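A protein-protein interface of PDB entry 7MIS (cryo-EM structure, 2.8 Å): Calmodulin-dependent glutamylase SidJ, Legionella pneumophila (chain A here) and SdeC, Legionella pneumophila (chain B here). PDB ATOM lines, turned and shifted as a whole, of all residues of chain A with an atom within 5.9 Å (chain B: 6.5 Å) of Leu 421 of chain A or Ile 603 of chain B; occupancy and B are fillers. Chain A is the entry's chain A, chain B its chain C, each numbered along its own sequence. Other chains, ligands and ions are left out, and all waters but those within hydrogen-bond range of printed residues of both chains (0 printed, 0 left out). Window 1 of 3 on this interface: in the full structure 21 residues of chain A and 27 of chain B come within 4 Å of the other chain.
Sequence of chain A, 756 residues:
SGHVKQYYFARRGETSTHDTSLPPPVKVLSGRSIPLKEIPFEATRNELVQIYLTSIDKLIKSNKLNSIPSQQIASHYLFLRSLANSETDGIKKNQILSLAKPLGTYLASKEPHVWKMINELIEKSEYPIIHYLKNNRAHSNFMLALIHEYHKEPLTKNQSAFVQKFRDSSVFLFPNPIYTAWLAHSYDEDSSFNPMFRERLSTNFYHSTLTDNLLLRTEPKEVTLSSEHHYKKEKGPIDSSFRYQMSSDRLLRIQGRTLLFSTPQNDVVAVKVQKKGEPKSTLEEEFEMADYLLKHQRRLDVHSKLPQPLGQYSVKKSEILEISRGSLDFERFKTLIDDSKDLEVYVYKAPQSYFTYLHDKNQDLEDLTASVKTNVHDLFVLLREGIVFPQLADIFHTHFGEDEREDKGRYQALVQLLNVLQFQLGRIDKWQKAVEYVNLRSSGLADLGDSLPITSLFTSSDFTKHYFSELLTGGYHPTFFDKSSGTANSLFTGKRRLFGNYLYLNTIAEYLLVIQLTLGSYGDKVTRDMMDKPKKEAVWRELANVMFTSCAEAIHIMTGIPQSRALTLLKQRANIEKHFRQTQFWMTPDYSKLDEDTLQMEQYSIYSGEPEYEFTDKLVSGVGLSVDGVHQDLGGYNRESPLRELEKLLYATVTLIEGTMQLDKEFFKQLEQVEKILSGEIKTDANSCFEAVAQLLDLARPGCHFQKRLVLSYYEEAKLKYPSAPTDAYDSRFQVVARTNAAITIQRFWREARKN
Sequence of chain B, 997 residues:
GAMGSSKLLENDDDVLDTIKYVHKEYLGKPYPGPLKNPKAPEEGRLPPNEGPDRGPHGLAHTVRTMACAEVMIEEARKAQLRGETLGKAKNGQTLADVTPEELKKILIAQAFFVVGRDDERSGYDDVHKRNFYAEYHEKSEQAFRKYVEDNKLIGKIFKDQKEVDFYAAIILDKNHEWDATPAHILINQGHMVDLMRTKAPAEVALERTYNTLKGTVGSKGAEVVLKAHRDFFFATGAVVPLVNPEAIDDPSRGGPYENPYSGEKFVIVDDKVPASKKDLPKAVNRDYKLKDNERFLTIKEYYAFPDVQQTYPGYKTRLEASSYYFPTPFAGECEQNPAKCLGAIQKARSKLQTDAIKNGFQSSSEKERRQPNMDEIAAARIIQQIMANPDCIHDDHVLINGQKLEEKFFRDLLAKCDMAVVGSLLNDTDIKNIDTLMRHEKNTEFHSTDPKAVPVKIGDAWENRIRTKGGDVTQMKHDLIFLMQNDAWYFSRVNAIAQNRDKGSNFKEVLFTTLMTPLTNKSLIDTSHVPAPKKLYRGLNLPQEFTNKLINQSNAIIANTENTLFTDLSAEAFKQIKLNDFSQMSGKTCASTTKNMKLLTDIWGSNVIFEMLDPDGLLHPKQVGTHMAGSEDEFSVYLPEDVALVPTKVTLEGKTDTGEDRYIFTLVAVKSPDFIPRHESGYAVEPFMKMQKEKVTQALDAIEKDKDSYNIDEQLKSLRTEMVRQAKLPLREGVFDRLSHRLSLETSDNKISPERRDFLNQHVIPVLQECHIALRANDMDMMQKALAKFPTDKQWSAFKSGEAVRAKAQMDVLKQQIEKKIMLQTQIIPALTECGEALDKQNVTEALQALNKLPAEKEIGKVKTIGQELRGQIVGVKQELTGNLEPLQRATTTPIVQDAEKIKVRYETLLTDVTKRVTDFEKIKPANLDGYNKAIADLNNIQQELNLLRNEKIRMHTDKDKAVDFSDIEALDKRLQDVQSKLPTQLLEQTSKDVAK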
ATOM      1  N   GLN A 164      11.888 -25.169   1.279  1.00  0.00           N
ATOM      2  CA  GLN A 164      11.671 -26.099   2.379  1.00  0.00           C
ATOM      3  C   GLN A 164      10.354 -25.852   3.098  1.00  0.00           C
ATOM      4  O   GLN A 164       9.872 -26.752   3.794  1.00  0.00           O
ATOM      5  CB  GLN A 164      12.819 -26.034   3.390  1.00  0.00           C
ATOM      6  CG  GLN A 164      12.954 -24.719   4.120  1.00  0.00           C
ATOM      7  CD  GLN A 164      14.144 -24.701   5.062  1.00  0.00           C
ATOM      8  OE1 GLN A 164      14.849 -25.701   5.210  1.00  0.00           O
ATOM      9  NE2 GLN A 164      14.376 -23.562   5.703  1.00  0.00           N
ATOM     10  N   ASN A 419       2.359 -19.592  14.821  1.00  0.00           N
ATOM     11  CA  ASN A 419       3.569 -19.948  15.544  1.00  0.00           C
ATOM     12  C   ASN A 419       4.620 -20.461  14.574  1.00  0.00           C
ATOM     13  O   ASN A 419       4.321 -20.849  13.443  1.00  0.00           O
ATOM     14  CB  ASN A 419       3.294 -21.012  16.612  1.00  0.00           C
ATOM     15  CG  ASN A 419       2.569 -20.456  17.814  1.00  0.00           C
ATOM     16  OD1 ASN A 419       3.190 -19.975  18.757  1.00  0.00           O
ATOM     17  ND2 ASN A 419       1.246 -20.518  17.786  1.00  0.00           N
ATOM     18  N   VAL A 420       5.861 -20.449  15.038  1.00  0.00           N
ATOM     19  CA  VAL A 420       6.977 -21.038  14.311  1.00  0.00           C
ATOM     20  C   VAL A 420       7.137 -22.481  14.767  1.00  0.00           C
ATOM     21  O   VAL A 420       7.162 -22.764  15.970  1.00  0.00           O
ATOM     22  CB  VAL A 420       8.271 -20.243  14.547  1.00  0.00           C
ATOM     23  CG1 VAL A 420       9.408 -20.839  13.747  1.00  0.00           C
ATOM     24  CG2 VAL A 420       8.080 -18.796  14.176  1.00  0.00           C
ATOM     25  N   LEU A 421       7.232 -23.395  13.806  1.00  0.00           N
ATOM     26  CA  LEU A 421       7.517 -24.799  14.087  1.00  0.00           C
ATOM     27  C   LEU A 421       6.466 -25.423  15.003  1.00  0.00           C
ATOM     28  O   LEU A 421       6.783 -26.212  15.894  1.00  0.00           O
ATOM     29  CB  LEU A 421       8.917 -24.957  14.683  1.00  0.00           C
ATOM     30  CG  LEU A 421      10.065 -24.591  13.741  1.00  0.00           C
ATOM     31  CD1 LEU A 421      11.392 -24.650  14.478  1.00  0.00           C
ATOM     32  CD2 LEU A 421      10.091 -25.486  12.513  1.00  0.00           C
ATOM     33  N   GLN A 422       5.206 -25.059  14.789  1.00  0.00           N
ATOM     34  CA  GLN A 422       4.064 -25.804  15.298  1.00  0.00           C
ATOM     35  C   GLN A 422       3.360 -26.440  14.109  1.00  0.00           C
ATOM     36  O   GLN A 422       3.209 -25.805  13.062  1.00  0.00           O
ATOM     37  CB  GLN A 422       3.095 -24.907  16.072  1.00  0.00           C
ATOM     38  CG  GLN A 422       3.700 -24.225  17.286  1.00  0.00           C
ATOM     39  CD  GLN A 422       3.883 -25.161  18.460  1.00  0.00           C
ATOM     40  OE1 GLN A 422       3.988 -26.374  18.294  1.00  0.00           O
ATOM     41  NE2 GLN A 422       3.931 -24.598  19.659  1.00  0.00           N
ATOM     42  N   PHE A 423       2.938 -27.694  14.262  1.00  0.00           N
ATOM     43  CA  PHE A 423       2.552 -28.495  13.112  1.00  0.00           C
ATOM     44  C   PHE A 423       1.132 -29.035  13.147  1.00  0.00           C
ATOM     45  O   PHE A 423       0.655 -29.504  12.109  1.00  0.00           O
ATOM     46  CB  PHE A 423       3.525 -29.673  12.948  1.00  0.00           C
ATOM     47  CG  PHE A 423       4.944 -29.246  12.730  1.00  0.00           C
ATOM     48  CD1 PHE A 423       5.330 -28.664  11.538  1.00  0.00           C
ATOM     49  CD2 PHE A 423       5.888 -29.405  13.726  1.00  0.00           C
ATOM     50  CE1 PHE A 423       6.632 -28.262  11.340  1.00  0.00           C
ATOM     51  CE2 PHE A 423       7.191 -29.005  13.531  1.00  0.00           C
ATOM     52  CZ  PHE A 423       7.563 -28.432  12.337  1.00  0.00           C
ATOM     53  N   GLU A 470       4.566 -13.993  19.888  1.00  0.00           N
ATOM     54  CA  GLU A 470       5.415 -14.629  18.890  1.00  0.00           C
ATOM     55  C   GLU A 470       5.093 -14.110  17.496  1.00  0.00           C
ATOM     56  O   GLU A 470       5.997 -13.836  16.701  1.00  0.00           O
ATOM     57  CB  GLU A 470       5.246 -16.145  18.945  1.00  0.00           C
ATOM     58  CG  GLU A 470       6.346 -16.908  18.230  1.00  0.00           C
ATOM     59  CD  GLU A 470       6.105 -18.403  18.213  1.00  0.00           C
ATOM     60  OE1 GLU A 470       5.975 -19.000  19.302  1.00  0.00           O
ATOM     61  OE2 GLU A 470       6.050 -18.981  17.108  1.00  0.00           O
ATOM     62  N   HIS A 477      14.847 -19.231  15.244  1.00  0.00           N
ATOM     63  CA  HIS A 477      15.313 -20.597  15.412  1.00  0.00           C
ATOM     64  C   HIS A 477      16.787 -20.623  15.037  1.00  0.00           C
ATOM     65  O   HIS A 477      17.203 -19.881  14.142  1.00  0.00           O
ATOM     66  CB  HIS A 477      14.524 -21.586  14.545  1.00  0.00           C
ATOM     67  CG  HIS A 477      14.688 -23.014  14.962  1.00  0.00           C
ATOM     68  ND1 HIS A 477      15.411 -23.926  14.225  1.00  0.00           N
ATOM     69  CD2 HIS A 477      14.232 -23.682  16.046  1.00  0.00           C
ATOM     70  CE1 HIS A 477      15.390 -25.096  14.837  1.00  0.00           C
ATOM     71  NE2 HIS A 477      14.682 -24.976  15.945  1.00  0.00           N
ATOM     72  N   THR A 479      18.597 -22.454  13.228  1.00  0.00           N
ATOM     73  CA  THR A 479      18.895 -22.701  11.824  1.00  0.00           C
ATOM     74  C   THR A 479      18.637 -21.481  10.950  1.00  0.00           C
ATOM     75  O   THR A 479      19.143 -21.425   9.824  1.00  0.00           O
ATOM     76  CB  THR A 479      18.075 -23.885  11.307  1.00  0.00           C
ATOM     77  OG1 THR A 479      16.680 -23.575  11.382  1.00  0.00           O
ATOM     78  CG2 THR A 479      18.365 -25.129  12.128  1.00  0.00           C
ATOM     79  N   PHE A 480      17.862 -20.505  11.432  1.00  0.00           N
ATOM     80  CA  PHE A 480      17.645 -19.282  10.667  1.00  0.00           C
ATOM     81  C   PHE A 480      18.861 -18.368  10.695  1.00  0.00           C
ATOM     82  O   PHE A 480      19.033 -17.558   9.779  1.00  0.00           O
ATOM     83  CB  PHE A 480      16.433 -18.517  11.206  1.00  0.00           C
ATOM     84  CG  PHE A 480      15.154 -19.309  11.214  1.00  0.00           C
ATOM     85  CD1 PHE A 480      14.974 -20.389  10.369  1.00  0.00           C
ATOM     86  CD2 PHE A 480      14.125 -18.963  12.072  1.00  0.00           C
ATOM     87  CE1 PHE A 480      13.796 -21.107  10.386  1.00  0.00           C
ATOM     88  CE2 PHE A 480      12.948 -19.679  12.090  1.00  0.00           C
ATOM     89  CZ  PHE A 480      12.784 -20.753  11.247  1.00  0.00           C
ATOM     90  N   ASN B 596       9.160 -36.148  16.294  1.00  0.00           N
ATOM     91  CA  ASN B 596       8.563 -35.513  15.120  1.00  0.00           C
ATOM     92  C   ASN B 596       9.602 -35.554  14.004  1.00  0.00           C
ATOM     93  O   ASN B 596      10.501 -34.710  13.954  1.00  0.00           O
ATOM     94  CB  ASN B 596       8.128 -34.084  15.423  1.00  0.00           C
ATOM     95  CG  ASN B 596       7.433 -33.426  14.249  1.00  0.00           C
ATOM     96  OD1 ASN B 596       7.495 -33.913  13.121  1.00  0.00           O
ATOM     97  ND2 ASN B 596       6.763 -32.313  14.509  1.00  0.00           N
ATOM     98  N   LYS B 598       9.328 -34.793  10.964  1.00  0.00           N
ATOM     99  CA  LYS B 598       9.284 -33.614  10.107  1.00  0.00           C
ATOM    100  C   LYS B 598      10.328 -32.594  10.534  1.00  0.00           C
ATOM    101  O   LYS B 598      10.909 -31.898   9.695  1.00  0.00           O
ATOM    102  CB  LYS B 598       7.887 -32.995  10.141  1.00  0.00           C
ATOM    103  CG  LYS B 598       7.752 -31.728   9.323  1.00  0.00           C
ATOM    104  CD  LYS B 598       6.369 -31.618   8.705  1.00  0.00           C
ATOM    105  CE  LYS B 598       6.069 -30.195   8.267  1.00  0.00           C
ATOM    106  NZ  LYS B 598       4.653 -30.028   7.845  1.00  0.00           N
ATOM    107  N   LEU B 599      10.587 -32.498  11.839  1.00  0.00           N
ATOM    108  CA  LEU B 599      11.580 -31.551  12.328  1.00  0.00           C
ATOM    109  C   LEU B 599      12.964 -31.874  11.776  1.00  0.00           C
ATOM    110  O   LEU B 599      13.701 -30.973  11.360  1.00  0.00           O
ATOM    111  CB  LEU B 599      11.590 -31.566  13.856  1.00  0.00           C
ATOM    112  CG  LEU B 599      11.910 -30.245  14.551  1.00  0.00           C
ATOM    113  CD1 LEU B 599      10.792 -29.243  14.330  1.00  0.00           C
ATOM    114  CD2 LEU B 599      12.137 -30.476  16.034  1.00  0.00           C
ATOM    115  N   LEU B 600      13.335 -33.154  11.764  1.00  0.00           N
ATOM    116  CA  LEU B 600      14.629 -33.539  11.211  1.00  0.00           C
ATOM    117  C   LEU B 600      14.659 -33.344   9.703  1.00  0.00           C
ATOM    118  O   LEU B 600      15.629 -32.810   9.154  1.00  0.00           O
ATOM    119  CB  LEU B 600      14.938 -34.995  11.560  1.00  0.00           C
ATOM    120  CG  LEU B 600      15.250 -35.311  13.020  1.00  0.00           C
ATOM    121  CD1 LEU B 600      15.414 -36.804  13.197  1.00  0.00           C
ATOM    122  CD2 LEU B 600      16.493 -34.579  13.478  1.00  0.00           C
ATOM    123  N   THR B 601      13.604 -33.777   9.014  1.00  0.00           N
ATOM    124  CA  THR B 601      13.611 -33.733   7.555  1.00  0.00           C
ATOM    125  C   THR B 601      13.661 -32.301   7.039  1.00  0.00           C
ATOM    126  O   THR B 601      14.394 -32.001   6.090  1.00  0.00           O
ATOM    127  CB  THR B 601      12.382 -34.454   7.001  1.00  0.00           C
ATOM    128  OG1 THR B 601      11.192 -33.823   7.486  1.00  0.00           O
ATOM    129  CG2 THR B 601      12.385 -35.917   7.412  1.00  0.00           C
ATOM    130  N   ASP B 602      12.891 -31.399   7.650  1.00  0.00           N
ATOM    131  CA  ASP B 602      12.709 -30.067   7.083  1.00  0.00           C
ATOM    132  C   ASP B 602      13.851 -29.124   7.448  1.00  0.00           C
ATOM    133  O   ASP B 602      14.589 -28.661   6.573  1.00  0.00           O
ATOM    134  CB  ASP B 602      11.374 -29.481   7.552  1.00  0.00           C
ATOM    135  CG  ASP B 602      10.196 -30.010   6.761  1.00  0.00           C
ATOM    136  OD1 ASP B 602      10.342 -31.061   6.103  1.00  0.00           O
ATOM    137  OD2 ASP B 602       9.123 -29.372   6.795  1.00  0.00           O
ATOM    138  N   ILE B 603      14.020 -28.838   8.735  1.00  0.00           N
ATOM    139  CA  ILE B 603      14.837 -27.716   9.173  1.00  0.00           C
ATOM    140  C   ILE B 603      16.243 -28.148   9.572  1.00  0.00           C
ATOM    141  O   ILE B 603      17.209 -27.436   9.297  1.00  0.00           O
ATOM    142  CB  ILE B 603      14.135 -26.961  10.324  1.00  0.00           C
ATOM    143  CG1 ILE B 603      13.998 -27.844  11.563  1.00  0.00           C
ATOM    144  CG2 ILE B 603      12.765 -26.487   9.875  1.00  0.00           C
ATOM    145  CD1 ILE B 603      13.399 -27.125  12.745  1.00  0.00           C
ATOM    146  N   TRP B 604      16.393 -29.303  10.217  1.00  0.00           N
ATOM    147  CA  TRP B 604      17.717 -29.731  10.647  1.00  0.00           C
ATOM    148  C   TRP B 604      18.539 -30.335   9.517  1.00  0.00           C
ATOM    149  O   TRP B 604      19.754 -30.491   9.677  1.00  0.00           O
ATOM    150  CB  TRP B 604      17.599 -30.732  11.798  1.00  0.00           C
ATOM    151  CG  TRP B 604      17.279 -30.083  13.111  1.00  0.00           C
ATOM    152  CD1 TRP B 604      16.147 -30.251  13.855  1.00  0.00           C
ATOM    153  CD2 TRP B 604      18.097 -29.155  13.833  1.00  0.00           C
ATOM    154  NE1 TRP B 604      16.211 -29.489  14.995  1.00  0.00           N
ATOM    155  CE2 TRP B 604      17.399 -28.806  15.006  1.00  0.00           C
ATOM    156  CE3 TRP B 604      19.352 -28.586  13.603  1.00  0.00           C
ATOM    157  CZ2 TRP B 604      17.913 -27.916  15.944  1.00  0.00           C
ATOM    158  CZ3 TRP B 604      19.861 -27.703  14.535  1.00  0.00           C
ATOM    159  CH2 TRP B 604      19.143 -27.377  15.692  1.00  0.00           C
ATOM    160  N   GLY B 605      17.916 -30.669   8.389  1.00  0.00           N
ATOM    161  CA  GLY B 605      18.637 -31.115   7.211  1.00  0.00           C
ATOM    162  C   GLY B 605      19.640 -32.219   7.466  1.00  0.00           C
ATOM    163  O   GLY B 605      20.848 -32.013   7.312  1.00  0.00           O
ATOM    164  N   SER B 606      19.156 -33.397   7.844  1.00  0.00           N
ATOM    165  CA  SER B 606      19.999 -34.547   8.138  1.00  0.00           C
ATOM    166  C   SER B 606      19.895 -35.561   7.009  1.00  0.00           C
ATOM    167  O   SER B 606      18.798 -35.848   6.520  1.00  0.00           O
ATOM    168  CB  SER B 606      19.589 -35.198   9.459  1.00  0.00           C
ATOM    169  OG  SER B 606      19.742 -34.294  10.538  1.00  0.00           O
ATOM    170  N   ALA B 629      11.804 -23.218  20.412  1.00  0.00           N
ATOM    171  CA  ALA B 629      10.862 -23.568  19.359  1.00  0.00           C
ATOM    172  C   ALA B 629      11.114 -24.987  18.865  1.00  0.00           C
ATOM    173  O   ALA B 629      12.239 -25.344  18.506  1.00  0.00           O
ATOM    174  CB  ALA B 629      10.974 -22.578  18.201  1.00  0.00           C
ATOM    175  N   GLY B 630      10.057 -25.795  18.850  1.00  0.00           N
ATOM    176  CA  GLY B 630      10.144 -27.163  18.391  1.00  0.00           C
ATOM    177  C   GLY B 630      10.737 -28.137  19.384  1.00  0.00           C
ATOM    178  O   GLY B 630      10.841 -29.328  19.065  1.00  0.00           O
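The side-chain amide oxygen (OE1) of Gln 164 of chain A sits close to the backbone carbonyl oxygen (O) of Asp 602 of chain B, at 3.3 Å.
A ring nitrogen (ND1) of His 477 of chain A lies within hydrogen-bond range of the side-chain hydroxyl of Thr 479 of chain A.
OD1 of Asn 596 of chain B lies within hydrogen-bond range of N of Lys 598 of chain B, 3.0 Å away.
OG1 of Thr 601 of chain B is in hydrogen-bond range of O of Lys 598 of chain B.
The backbone carbonyl oxygen of Leu 599 of chain B lies within hydrogen-bond range of the backbone NH of Trp 604 of chain B, 3.4 Å away.
OG1 of Thr 601 of chain B is in hydrogen-bond range of OD1 of Asp 602 of chain B (3.2 Å).
CD1 of Leu 421 of chain A touches CD1 of Ile 603 of chain B (3.6 Å).
ND2 of Asn 596 of chain B touches CD2 of Phe 423 of chain A, at 3.1 Å.
Phe 423 of chain A touches Lys 598 of chain B.
CE2 of Phe 423 of chain A touches CD1 of Leu 599 of chain B, 3.7 Å away.
His 477 of chain A touches Ile 603 of chain B (CE1 to CD1, 3.5 Å).
Trp 604 of chain B touches His 477 of chain A (CZ2 to CE1, 3.9 Å).
His 477 of chain A touches Ala 629 of chain B.
O of Ile 603 of chain B touches CG2 of Thr 479 of chain A, 3.8 Å away.
CZ3 of Trp 604 of chain B touches CG2 of Thr 479 of chain A, at 3.8 Å.
Printed residues of chain B within 4 Å of Gln 164 of chain A: Asp 602 (3.3 Å).
Leu 421 of chain A touches just one residue of chain B: Ile 603.
Glu 470 of chain A touches none of the printed residues of chain B.
Of the printed residues of chain B, His 477 of chain A touches Ile 603, Trp 604 and Ala 629.
Ser 606 of chain B touches none of the printed residues of chain A.
Of the 12 printed residues of chain B, 7 touch a printed residue of chain A.
Hydrophobic or aromatic side chains of chain B that line the printed part of chain A: Leu 599, Ile 603 and Trp 604.
Hydrophobic or aromatic side chains of chain A that line the printed part of chain B: Leu 421, Phe 423 and His 477.
Along chain A the printed residues that touch a printed residue of chain B span positions 164 to 479.
Among the printed residues, 10 pairs touch across the chains.
Among the printed residues, no Asp or Glu carboxylate lies within 4 Å of a Lys or Arg side-chain nitrogen of the other chain.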
